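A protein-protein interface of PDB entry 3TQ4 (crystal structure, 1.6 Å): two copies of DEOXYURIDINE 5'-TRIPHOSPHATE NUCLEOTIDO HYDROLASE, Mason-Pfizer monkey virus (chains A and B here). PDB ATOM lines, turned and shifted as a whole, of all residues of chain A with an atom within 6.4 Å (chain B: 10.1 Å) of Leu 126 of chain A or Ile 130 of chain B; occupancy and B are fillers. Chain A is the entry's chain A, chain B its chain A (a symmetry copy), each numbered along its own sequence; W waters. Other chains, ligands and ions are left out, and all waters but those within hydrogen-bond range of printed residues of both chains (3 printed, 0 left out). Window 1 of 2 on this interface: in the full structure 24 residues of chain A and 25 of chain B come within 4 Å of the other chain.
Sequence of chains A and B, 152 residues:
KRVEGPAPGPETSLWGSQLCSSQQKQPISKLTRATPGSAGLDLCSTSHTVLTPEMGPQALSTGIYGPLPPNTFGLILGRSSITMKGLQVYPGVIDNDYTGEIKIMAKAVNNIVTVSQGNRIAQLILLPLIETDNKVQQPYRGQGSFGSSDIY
ND2 of Asn 134 of chain B is in hydrogen-bond range of O of Ile 28 of chain A (2.9 Å).
The guanidinium group (NH2) of Arg 33 of chain A sits at hydrogen-bond distance from the side-chain hydroxyl (OG1) of Thr 132 of chain B (2.9 Å).
The guanidinium group of Arg 33 of chain A is in hydrogen-bond range of the backbone carbonyl oxygen of Ala 39 of chain A.
The backbone NH (N) of Leu 124 of chain A sits at hydrogen-bond distance from the backbone carbonyl oxygen (O) of Leu 41 of chain A, at 2.8 Å.
The backbone NH (N) of Leu 75 of chain A sits at hydrogen-bond distance from the backbone carbonyl oxygen (O) of Ile 125 of chain A, 2.8 Å away.
The backbone carbonyl oxygen (O) of Asn 71 of chain B sits at hydrogen-bond distance from the backbone NH (N) of Leu 129 of chain B, at 2.9 Å.
N of Phe 73 of chain B lies within hydrogen-bond range of O of Leu 127 of chain B.
The side-chain hydroxyl (OG1) of Thr 132 of chain B is in hydrogen-bond range of the side-chain amide oxygen (OD1) of Asn 134 of chain B (2.5 Å).
Among the printed residues, merely in contact across the chains: Ala 39 of chain A with Phe 73 of chain B (3.6 Å), Ala 39 of chain A with Val 93 of chain B (3.7 Å), Ala 39 of chain A with Leu 129 of chain B (3.6 Å), Leu 41 of chain A with Asn 134 of chain B (3.6 Å), Ile 125 of chain A with Phe 73 of chain B (3.6 Å), Ile 125 of chain A with Val 93 of chain B (3.7 Å), Leu 126 of chain A with Ile 130 of chain B (3.6 Å), Leu 126 of chain A with Thr 132 of chain B (3.6 Å), Leu 127 of chain A with Phe 73 of chain B (3.9 Å), Leu 127 of chain A with Ile 130 of chain B (3.7 Å), Pro 128 of chain A with Pro 128 of chain B (3.8 Å) and Pro 128 of chain A with Ile 130 of chain B (3.8 Å).
Of chain B, only Phe 73 (3.6 Å) and Val 93 (3.7 Å) come within 4 Å of Ile 125 of chain A.
Of chain B, only Ile 130 (3.6 Å) and Thr 132 (3.6 Å) come within 4 Å of Leu 126 of chain A.
Leu 127 of chain A touches just these residues of chain B: Phe 73 (3.9 Å) and Ile 130 (3.7 Å).
Of the printed residues of chain A, Pro 128 of chain B touches Pro 128 (3.8 Å).
Ile 130 of chain B touches just these residues of chain A: Leu 126, Leu 127 and Pro 128.
Of the printed residues of chain A, Thr 132 of chain B touches Arg 33 (2.9 Å) and Leu 126 (3.6 Å).
Printed residues of chain A within 4 Å of Asn 134 of chain B: Ile 28 (2.9 Å) and Leu 41 (3.6 Å).
The nearest residue of chain B that does not touch Leu 126 of chain A is Pro 128 of chain B (4.6 Å).
The nearest residue of chain A that does not touch Ile 130 of chain B is Thr 72 of chain A (4.1 Å).
Of the 16 printed residues of chain B, 7 touch a printed residue of chain A.
Printed residues of chain A that touch a printed residue of chain B: Ile 28, Arg 33, Ala 39, Leu 41, Ile 125, Leu 126, Leu 127 and Pro 128.
Leu 127 of chain A touches Phe 73 of chain B, but with the chains exchanged Phe 73 of chain A does not touch Leu 127 of chain B (7.7 Å).
Pro 128 of chain B touches its own counterpart, Pro 128 of chain A.
Of the 14 pairs that touch across the chains among the printed residues, 1 has its exchanged pair printed and touching as well.
Water W1 lies within hydrogen-bond range of the backbone carbonyl oxygen (O) of Leu 126 of chain A (2.5 Å), the backbone NH (N) of Ile 130 of chain B (2.8 Å) and the backbone carbonyl oxygen (O) of Pro 128 of chain B (2.9 Å).
Water W2 lies within hydrogen-bond range of NE of Arg 33 of chain A, O of Asn 134 of chain B and O of Thr 132 of chain B.
Water W3 lies within hydrogen-bond range of the guanidinium group (NH2) of Arg 33 of chain A (2.8 Å) and the backbone carbonyl oxygen (O) of Ile 130 of chain B (2.9 Å).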
ATOM      1  N   ILE A  28     -18.849 -31.613  -4.454  1.00  0.00           N
ATOM      2  CA  ILE A  28     -18.128 -30.764  -5.411  1.00  0.00           C
ATOM      3  C   ILE A  28     -19.071 -30.021  -6.364  1.00  0.00           C
ATOM      4  O   ILE A  28     -18.808 -28.888  -6.812  1.00  0.00           O
ATOM      5  CB  ILE A  28     -17.118 -31.711  -6.204  1.00  0.00           C
ATOM      6  CG1 ILE A  28     -16.039 -32.209  -5.240  1.00  0.00           C
ATOM      7  CG2 ILE A  28     -16.538 -31.114  -7.492  1.00  0.00           C
ATOM      8  CD1 ILE A  28     -15.583 -31.181  -4.228  1.00  0.00           C
ATOM      9  N   ARG A  33     -18.138 -21.430 -10.269  1.00  0.00           N
ATOM     10  CA  ARG A  33     -17.073 -20.778 -11.040  1.00  0.00           C
ATOM     11  C   ARG A  33     -17.392 -19.309 -11.061  1.00  0.00           C
ATOM     12  O   ARG A  33     -18.567 -18.959 -11.213  1.00  0.00           O
ATOM     13  CB  ARG A  33     -17.161 -21.212 -12.501  1.00  0.00           C
ATOM     14  CG  ARG A  33     -16.309 -22.303 -12.838  1.00  0.00           C
ATOM     15  CD  ARG A  33     -16.321 -22.714 -14.300  1.00  0.00           C
ATOM     16  NE  ARG A  33     -16.306 -24.183 -14.188  1.00  0.00           N
ATOM     17  CZ  ARG A  33     -15.261 -24.943 -13.829  1.00  0.00           C
ATOM     18  NH1 ARG A  33     -14.063 -24.413 -13.621  1.00  0.00           N
ATOM     19  NH2 ARG A  33     -15.420 -26.259 -13.682  1.00  0.00           N
ATOM     20  N   ALA A  39     -10.761 -21.346 -14.476  1.00  0.00           N
ATOM     21  CA  ALA A  39     -10.243 -22.665 -14.455  1.00  0.00           C
ATOM     22  C   ALA A  39     -10.690 -23.299 -13.140  1.00  0.00           C
ATOM     23  O   ALA A  39     -10.865 -24.521 -13.049  1.00  0.00           O
ATOM     24  CB  ALA A  39      -8.758 -22.604 -14.541  1.00  0.00           C
ATOM     25  N   GLY A  40     -10.931 -22.487 -12.116  1.00  0.00           N
ATOM     26  CA  GLY A  40     -11.128 -23.057 -10.782  1.00  0.00           C
ATOM     27  C   GLY A  40     -12.518 -22.917 -10.219  1.00  0.00           C
ATOM     28  O   GLY A  40     -13.280 -22.003 -10.584  1.00  0.00           O
ATOM     29  N   LEU A  41     -12.853 -23.867  -9.340  1.00  0.00           N
ATOM     30  CA  LEU A  41     -14.092 -23.763  -8.544  1.00  0.00           C
ATOM     31  C   LEU A  41     -13.770 -23.137  -7.206  1.00  0.00           C
ATOM     32  O   LEU A  41     -12.848 -23.547  -6.545  1.00  0.00           O
ATOM     33  CB  LEU A  41     -14.637 -25.156  -8.324  1.00  0.00           C
ATOM     34  CG  LEU A  41     -15.085 -25.863  -9.604  1.00  0.00           C
ATOM     35  CD1 LEU A  41     -15.457 -27.327  -9.249  1.00  0.00           C
ATOM     36  CD2 LEU A  41     -16.277 -25.184 -10.223  1.00  0.00           C
ATOM     37  N   LEU A  68     -14.487 -37.118  -6.537  1.00  0.00           N
ATOM     38  CA  LEU A  68     -14.450 -36.357  -7.764  1.00  0.00           C
ATOM     39  C   LEU A  68     -15.078 -37.165  -8.895  1.00  0.00           C
ATOM     40  O   LEU A  68     -15.365 -38.352  -8.731  1.00  0.00           O
ATOM     41  CB  LEU A  68     -13.003 -36.047  -8.053  1.00  0.00           C
ATOM     42  CG  LEU A  68     -12.518 -34.781  -7.347  1.00  0.00           C
ATOM     43  CD1 LEU A  68     -12.717 -34.777  -5.904  1.00  0.00           C
ATOM     44  CD2 LEU A  68     -11.081 -34.637  -7.550  1.00  0.00           C
ATOM     45  N   PRO A  69     -15.366 -36.506 -10.027  1.00  0.00           N
ATOM     46  CA  PRO A  69     -15.864 -37.133 -11.223  1.00  0.00           C
ATOM     47  C   PRO A  69     -14.907 -38.218 -11.693  1.00  0.00           C
ATOM     48  O   PRO A  69     -13.673 -38.115 -11.461  1.00  0.00           O
ATOM     49  CB  PRO A  69     -15.844 -35.986 -12.241  1.00  0.00           C
ATOM     50  CG  PRO A  69     -16.061 -34.777 -11.438  1.00  0.00           C
ATOM     51  CD  PRO A  69     -15.252 -35.039 -10.186  1.00  0.00           C
ATOM     52  N   ASN A  71     -12.259 -40.457 -13.479  1.00  0.00           N
ATOM     53  CA  ASN A  71     -11.075 -40.133 -14.283  1.00  0.00           C
ATOM     54  C   ASN A  71     -10.503 -38.737 -14.057  1.00  0.00           C
ATOM     55  O   ASN A  71      -9.815 -38.221 -14.938  1.00  0.00           O
ATOM     56  CB  ASN A  71     -11.361 -40.305 -15.783  1.00  0.00           C
ATOM     57  CG  ASN A  71     -11.984 -41.656 -16.094  1.00  0.00           C
ATOM     58  OD1 ASN A  71     -11.426 -42.702 -15.764  1.00  0.00           O
ATOM     59  ND2 ASN A  71     -13.167 -41.635 -16.706  1.00  0.00           N
ATOM     60  N   THR A  72     -10.825 -38.119 -12.928  1.00  0.00           N
ATOM     61  CA  THR A  72     -10.262 -36.787 -12.633  1.00  0.00           C
ATOM     62  C   THR A  72      -9.649 -36.800 -11.244  1.00  0.00           C
ATOM     63  O   THR A  72     -10.018 -37.644 -10.392  1.00  0.00           O
ATOM     64  CB  THR A  72     -11.307 -35.608 -12.647  1.00  0.00           C
ATOM     65  OG1 THR A  72     -12.167 -35.741 -11.503  1.00  0.00           O
ATOM     66  CG2 THR A  72     -12.159 -35.570 -13.961  1.00  0.00           C
ATOM     67  N   PHE A  73      -8.710 -35.880 -11.011  1.00  0.00           N
ATOM     68  CA  PHE A  73      -8.267 -35.631  -9.648  1.00  0.00           C
ATOM     69  C   PHE A  73      -8.291 -34.112  -9.453  1.00  0.00           C
ATOM     70  O   PHE A  73      -8.501 -33.349 -10.409  1.00  0.00           O
ATOM     71  CB  PHE A  73      -6.874 -36.261  -9.349  1.00  0.00           C
ATOM     72  CG  PHE A  73      -5.720 -35.511  -9.972  1.00  0.00           C
ATOM     73  CD1 PHE A  73      -4.996 -34.555  -9.220  1.00  0.00           C
ATOM     74  CD2 PHE A  73      -5.381 -35.670 -11.301  1.00  0.00           C
ATOM     75  CE1 PHE A  73      -3.945 -33.845  -9.798  1.00  0.00           C
ATOM     76  CE2 PHE A  73      -4.293 -34.935 -11.853  1.00  0.00           C
ATOM     77  CZ  PHE A  73      -3.649 -34.031 -11.127  1.00  0.00           C
ATOM     78  N   GLY A  74      -8.097 -33.673  -8.217  1.00  0.00           N
ATOM     79  CA  GLY A  74      -8.224 -32.208  -7.927  1.00  0.00           C
ATOM     80  C   GLY A  74      -6.910 -31.644  -7.448  1.00  0.00           C
ATOM     81  O   GLY A  74      -6.068 -32.350  -6.867  1.00  0.00           O
ATOM     82  N   LEU A  75      -6.733 -30.364  -7.728  1.00  0.00           N
ATOM     83  CA  LEU A  75      -5.640 -29.627  -7.131  1.00  0.00           C
ATOM     84  C   LEU A  75      -6.214 -28.362  -6.467  1.00  0.00           C
ATOM     85  O   LEU A  75      -6.931 -27.624  -7.101  1.00  0.00           O
ATOM     86  CB  LEU A  75      -4.688 -29.211  -8.243  1.00  0.00           C
ATOM     87  CG  LEU A  75      -3.210 -29.016  -7.989  1.00  0.00           C
ATOM     88  CD1 LEU A  75      -2.608 -30.316  -7.372  1.00  0.00           C
ATOM     89  CD2 LEU A  75      -2.537 -28.575  -9.324  1.00  0.00           C
ATOM     90  N   LEU A 124     -10.470 -24.947  -6.515  1.00  0.00           N
ATOM     91  CA  LEU A 124     -10.271 -26.336  -6.876  1.00  0.00           C
ATOM     92  C   LEU A 124     -10.193 -26.424  -8.398  1.00  0.00           C
ATOM     93  O   LEU A 124     -11.161 -26.080  -9.098  1.00  0.00           O
ATOM     94  CB  LEU A 124     -11.477 -27.175  -6.378  1.00  0.00           C
ATOM     95  CG  LEU A 124     -11.372 -28.662  -6.744  1.00  0.00           C
ATOM     96  CD1 LEU A 124     -10.195 -29.374  -6.033  1.00  0.00           C
ATOM     97  CD2 LEU A 124     -12.677 -29.315  -6.239  1.00  0.00           C
ATOM     98  N   ILE A 125      -9.069 -26.943  -8.896  1.00  0.00           N
ATOM     99  CA  ILE A 125      -8.874 -27.233 -10.327  1.00  0.00           C
ATOM    100  C   ILE A 125      -9.040 -28.767 -10.561  1.00  0.00           C
ATOM    101  O   ILE A 125      -8.589 -29.589  -9.741  1.00  0.00           O
ATOM    102  CB  ILE A 125      -7.467 -26.700 -10.767  1.00  0.00           C
ATOM    103  CG1 ILE A 125      -7.542 -25.176 -11.070  1.00  0.00           C
ATOM    104  CG2 ILE A 125      -6.867 -27.513 -11.905  1.00  0.00           C
ATOM    105  CD1 ILE A 125      -7.397 -24.330  -9.910  1.00  0.00           C
ATOM    106  N   LEU A 126      -9.749 -29.151 -11.622  1.00  0.00           N
ATOM    107  CA  LEU A 126      -9.930 -30.588 -11.955  1.00  0.00           C
ATOM    108  C   LEU A 126      -9.035 -30.908 -13.132  1.00  0.00           C
ATOM    109  O   LEU A 126      -8.947 -30.132 -14.106  1.00  0.00           O
ATOM    110  CB  LEU A 126     -11.375 -30.881 -12.277  1.00  0.00           C
ATOM    111  CG  LEU A 126     -12.339 -30.641 -11.133  1.00  0.00           C
ATOM    112  CD1 LEU A 126     -13.742 -30.924 -11.670  1.00  0.00           C
ATOM    113  CD2 LEU A 126     -12.051 -31.559  -9.902  1.00  0.00           C
ATOM    114  N   LEU A 127      -8.340 -32.046 -13.019  1.00  0.00           N
ATOM    115  CA  LEU A 127      -7.361 -32.444 -14.017  1.00  0.00           C
ATOM    116  C   LEU A 127      -7.562 -33.926 -14.345  1.00  0.00           C
ATOM    117  O   LEU A 127      -8.067 -34.705 -13.509  1.00  0.00           O
ATOM    118  CB  LEU A 127      -5.958 -32.226 -13.474  1.00  0.00           C
ATOM    119  CG  LEU A 127      -5.521 -30.739 -13.450  1.00  0.00           C
ATOM    120  CD1 LEU A 127      -4.290 -30.564 -12.597  1.00  0.00           C
ATOM    121  CD2 LEU A 127      -5.354 -30.157 -14.884  1.00  0.00           C
ATOM    122  N   PRO A 128      -7.154 -34.326 -15.555  1.00  0.00           N
ATOM    123  CA  PRO A 128      -7.334 -35.727 -15.935  1.00  0.00           C
ATOM    124  C   PRO A 128      -6.432 -36.619 -15.104  1.00  0.00           C
ATOM    125  O   PRO A 128      -5.321 -36.234 -14.753  1.00  0.00           O
ATOM    126  CB  PRO A 128      -6.880 -35.758 -17.409  1.00  0.00           C
ATOM    127  CG  PRO A 128      -5.977 -34.585 -17.573  1.00  0.00           C
ATOM    128  CD  PRO A 128      -6.531 -33.518 -16.631  1.00  0.00           C
ATOM    129  N   PRO B  70      -7.965 -22.165 -26.941  1.00  0.00           N
ATOM    130  CA  PRO B  70      -9.245 -22.715 -26.503  1.00  0.00           C
ATOM    131  C   PRO B  70      -9.069 -24.016 -25.721  1.00  0.00           C
ATOM    132  O   PRO B  70      -8.160 -24.832 -25.985  1.00  0.00           O
ATOM    133  CB  PRO B  70     -10.047 -22.901 -27.802  1.00  0.00           C
ATOM    134  CG  PRO B  70      -9.132 -22.601 -28.861  1.00  0.00           C
ATOM    135  CD  PRO B  70      -7.950 -21.892 -28.391  1.00  0.00           C
ATOM    136  N   ASN B  71      -9.921 -24.172 -24.724  1.00  0.00           N
ATOM    137  CA  ASN B  71      -9.944 -25.395 -23.913  1.00  0.00           C
ATOM    138  C   ASN B  71      -8.698 -25.631 -23.065  1.00  0.00           C
ATOM    139  O   ASN B  71      -8.429 -26.775 -22.698  1.00  0.00           O
ATOM    140  CB  ASN B  71     -10.177 -26.636 -24.790  1.00  0.00           C
ATOM    141  CG  ASN B  71     -11.374 -26.467 -25.710  1.00  0.00           C
ATOM    142  OD1 ASN B  71     -12.486 -26.193 -25.259  1.00  0.00           O
ATOM    143  ND2 ASN B  71     -11.141 -26.599 -27.015  1.00  0.00           N
ATOM    144  N   THR B  72      -7.927 -24.583 -22.804  1.00  0.00           N
ATOM    145  CA  THR B  72      -6.736 -24.740 -21.948  1.00  0.00           C
ATOM    146  C   THR B  72      -6.765 -23.690 -20.851  1.00  0.00           C
ATOM    147  O   THR B  72      -7.427 -22.634 -20.998  1.00  0.00           O
ATOM    148  CB  THR B  72      -5.358 -24.568 -22.691  1.00  0.00           C
ATOM    149  OG1 THR B  72      -5.193 -23.185 -23.043  1.00  0.00           O
ATOM    150  CG2 THR B  72      -5.243 -25.467 -23.969  1.00  0.00           C
ATOM    151  N   PHE B  73      -6.064 -23.974 -19.751  1.00  0.00           N
ATOM    152  CA  PHE B  73      -5.803 -22.930 -18.773  1.00  0.00           C
ATOM    153  C   PHE B  73      -4.307 -22.996 -18.453  1.00  0.00           C
ATOM    154  O   PHE B  73      -3.603 -23.922 -18.885  1.00  0.00           O
ATOM    155  CB  PHE B  73      -6.703 -23.059 -17.508  1.00  0.00           C
ATOM    156  CG  PHE B  73      -6.288 -24.177 -16.579  1.00  0.00           C
ATOM    157  CD1 PHE B  73      -5.459 -23.913 -15.463  1.00  0.00           C
ATOM    158  CD2 PHE B  73      -6.635 -25.491 -16.822  1.00  0.00           C
ATOM    159  CE1 PHE B  73      -5.057 -24.945 -14.618  1.00  0.00           C
ATOM    160  CE2 PHE B  73      -6.216 -26.517 -15.928  1.00  0.00           C
ATOM    161  CZ  PHE B  73      -5.420 -26.239 -14.904  1.00  0.00           C
ATOM    162  N   GLY B  74      -3.817 -22.009 -17.717  1.00  0.00           N
ATOM    163  CA  GLY B  74      -2.341 -21.941 -17.462  1.00  0.00           C
ATOM    164  C   GLY B  74      -2.049 -22.077 -15.989  1.00  0.00           C
ATOM    165  O   GLY B  74      -2.872 -21.734 -15.124  1.00  0.00           O
ATOM    166  N   LEU B  75      -0.870 -22.612 -15.716  1.00  0.00           N
ATOM    167  CA  LEU B  75      -0.350 -22.588 -14.366  1.00  0.00           C
ATOM    168  C   LEU B  75       1.065 -21.981 -14.403  1.00  0.00           C
ATOM    169  O   LEU B  75       1.887 -22.423 -15.170  1.00  0.00           O
ATOM    170  CB  LEU B  75      -0.257 -24.023 -13.870  1.00  0.00           C
ATOM    171  CG  LEU B  75      -0.380 -24.364 -12.401  1.00  0.00           C
ATOM    172  CD1 LEU B  75      -1.722 -23.802 -11.843  1.00  0.00           C
ATOM    173  CD2 LEU B  75      -0.218 -25.906 -12.241  1.00  0.00           C
ATOM    174  N   VAL B  93      -2.928 -19.597 -11.131  1.00  0.00           N
ATOM    175  CA  VAL B  93      -3.825 -20.161 -12.131  1.00  0.00           C
ATOM    176  C   VAL B  93      -4.080 -19.040 -13.131  1.00  0.00           C
ATOM    177  O   VAL B  93      -4.475 -17.927 -12.746  1.00  0.00           O
ATOM    178  CB  VAL B  93      -5.163 -20.565 -11.464  1.00  0.00           C
ATOM    179  CG1 VAL B  93      -6.171 -20.967 -12.484  1.00  0.00           C
ATOM    180  CG2 VAL B  93      -4.904 -21.715 -10.502  1.00  0.00           C
ATOM    181  N   ASN B  96      -8.617 -19.242 -18.707  1.00  0.00           N
ATOM    182  CA  ASN B  96      -8.651 -19.259 -20.204  1.00  0.00           C
ATOM    183  C   ASN B  96      -8.898 -17.928 -20.828  1.00  0.00           C
ATOM    184  O   ASN B  96      -8.320 -17.605 -21.902  1.00  0.00           O
ATOM    185  CB  ASN B  96      -9.710 -20.250 -20.701  1.00  0.00           C
ATOM    186  CG  ASN B  96      -9.744 -20.332 -22.207  1.00  0.00           C
ATOM    187  OD1 ASN B  96     -10.620 -19.753 -22.845  1.00  0.00           O
ATOM    188  ND2 ASN B  96      -8.749 -20.977 -22.794  1.00  0.00           N
ATOM    189  N   LEU B 127      -2.601 -26.589 -19.536  1.00  0.00           N
ATOM    190  CA  LEU B 127      -3.295 -27.794 -19.113  1.00  0.00           C
ATOM    191  C   LEU B 127      -4.717 -27.774 -19.682  1.00  0.00           C
ATOM    192  O   LEU B 127      -5.285 -26.693 -19.946  1.00  0.00           O
ATOM    193  CB  LEU B 127      -3.353 -27.846 -17.596  1.00  0.00           C
ATOM    194  CG  LEU B 127      -2.006 -28.231 -16.932  1.00  0.00           C
ATOM    195  CD1 LEU B 127      -2.040 -27.930 -15.454  1.00  0.00           C
ATOM    196  CD2 LEU B 127      -1.604 -29.704 -17.242  1.00  0.00           C
ATOM    197  N   PRO B 128      -5.302 -28.963 -19.858  1.00  0.00           N
ATOM    198  CA  PRO B 128      -6.655 -29.011 -20.414  1.00  0.00           C
ATOM    199  C   PRO B 128      -7.651 -28.431 -19.429  1.00  0.00           C
ATOM    200  O   PRO B 128      -7.497 -28.580 -18.221  1.00  0.00           O
ATOM    201  CB  PRO B 128      -6.915 -30.521 -20.588  1.00  0.00           C
ATOM    202  CG  PRO B 128      -5.994 -31.198 -19.633  1.00  0.00           C
ATOM    203  CD  PRO B 128      -4.752 -30.311 -19.577  1.00  0.00           C
ATOM    204  N   LEU B 129      -8.640 -27.713 -19.959  1.00  0.00           N
ATOM    205  CA  LEU B 129      -9.660 -27.178 -19.086  1.00  0.00           C
ATOM    206  C   LEU B 129     -10.841 -28.127 -19.165  1.00  0.00           C
ATOM    207  O   LEU B 129     -11.509 -28.181 -20.187  1.00  0.00           O
ATOM    208  CB  LEU B 129     -10.042 -25.777 -19.539  1.00  0.00           C
ATOM    209  CG  LEU B 129     -11.055 -24.973 -18.733  1.00  0.00           C
ATOM    210  CD1 LEU B 129     -10.648 -24.795 -17.323  1.00  0.00           C
ATOM    211  CD2 LEU B 129     -11.114 -23.626 -19.431  1.00  0.00           C
ATOM    212  N   ILE B 130     -11.093 -28.873 -18.082  1.00  0.00           N
ATOM    213  CA  ILE B 130     -12.206 -29.793 -18.029  1.00  0.00           C
ATOM    214  C   ILE B 130     -13.533 -29.047 -17.875  1.00  0.00           C
ATOM    215  O   ILE B 130     -13.662 -28.154 -17.040  1.00  0.00           O
ATOM    216  CB  ILE B 130     -11.978 -30.797 -16.893  1.00  0.00           C
ATOM    217  CG1 ILE B 130     -10.842 -31.732 -17.288  1.00  0.00           C
ATOM    218  CG2 ILE B 130     -13.223 -31.577 -16.553  1.00  0.00           C
ATOM    219  CD1 ILE B 130     -10.438 -32.593 -16.187  1.00  0.00           C
ATOM    220  N   GLU B 131     -14.529 -29.430 -18.683  1.00  0.00           N
ATOM    221  CA  GLU B 131     -15.911 -28.951 -18.519  1.00  0.00           C
ATOM    222  C   GLU B 131     -16.659 -29.692 -17.372  1.00  0.00           C
ATOM    223  O   GLU B 131     -16.483 -30.901 -17.158  1.00  0.00           O
ATOM    224  CB  GLU B 131     -16.663 -29.088 -19.867  1.00  0.00           C
ATOM    225  CG  GLU B 131     -16.179 -28.187 -21.008  1.00  0.00           C
ATOM    226  N   THR B 132     -17.464 -28.961 -16.602  1.00  0.00           N
ATOM    227  CA  THR B 132     -18.298 -29.564 -15.551  1.00  0.00           C
ATOM    228  C   THR B 132     -19.648 -28.857 -15.599  1.00  0.00           C
ATOM    229  O   THR B 132     -19.765 -27.830 -16.244  1.00  0.00           O
ATOM    230  CB  THR B 132     -17.679 -29.389 -14.118  1.00  0.00           C
ATOM    231  OG1 THR B 132     -17.731 -28.005 -13.707  1.00  0.00           O
ATOM    232  CG2 THR B 132     -16.222 -29.874 -14.070  1.00  0.00           C
ATOM    233  N   ASP B 133     -20.645 -29.381 -14.902  1.00  0.00           N
ATOM    234  CA  ASP B 133     -21.956 -28.733 -14.836  1.00  0.00           C
ATOM    235  C   ASP B 133     -22.017 -27.707 -13.711  1.00  0.00           C
ATOM    236  O   ASP B 133     -23.101 -27.251 -13.376  1.00  0.00           O
ATOM    237  CB  ASP B 133     -23.069 -29.775 -14.623  1.00  0.00           C
ATOM    238  CG  ASP B 133     -23.310 -30.660 -15.861  1.00  0.00           C
ATOM    239  OD1 ASP B 133     -23.239 -31.910 -15.743  1.00  0.00           O
ATOM    240  OD2 ASP B 133     -23.582 -30.103 -16.951  1.00  0.00           O
ATOM    241  N   ASN B 134     -20.874 -27.362 -13.093  1.00  0.00           N
ATOM    242  CA  ASN B 134     -20.916 -26.385 -12.002  1.00  0.00           C
ATOM    243  C   ASN B 134     -21.513 -25.052 -12.447  1.00  0.00           C
ATOM    244  O   ASN B 134     -21.188 -24.555 -13.529  1.00  0.00           O
ATOM    245  CB  ASN B 134     -19.542 -26.167 -11.362  1.00  0.00           C
ATOM    246  CG  ASN B 134     -19.025 -27.412 -10.670  1.00  0.00           C
ATOM    247  OD1 ASN B 134     -18.420 -28.272 -11.323  1.00  0.00           O
ATOM    248  ND2 ASN B 134     -19.228 -27.509  -9.355  1.00  0.00           N
HETATM  249  O   HOH W   1      -9.267 -28.423 -15.958  1.00  0.00           O
HETATM  250  O   HOH W   2     -18.646 -25.168 -14.983  1.00  0.00           O
HETATM  251  O   HOH W   3     -13.137 -27.672 -14.278  1.00  0.00           O
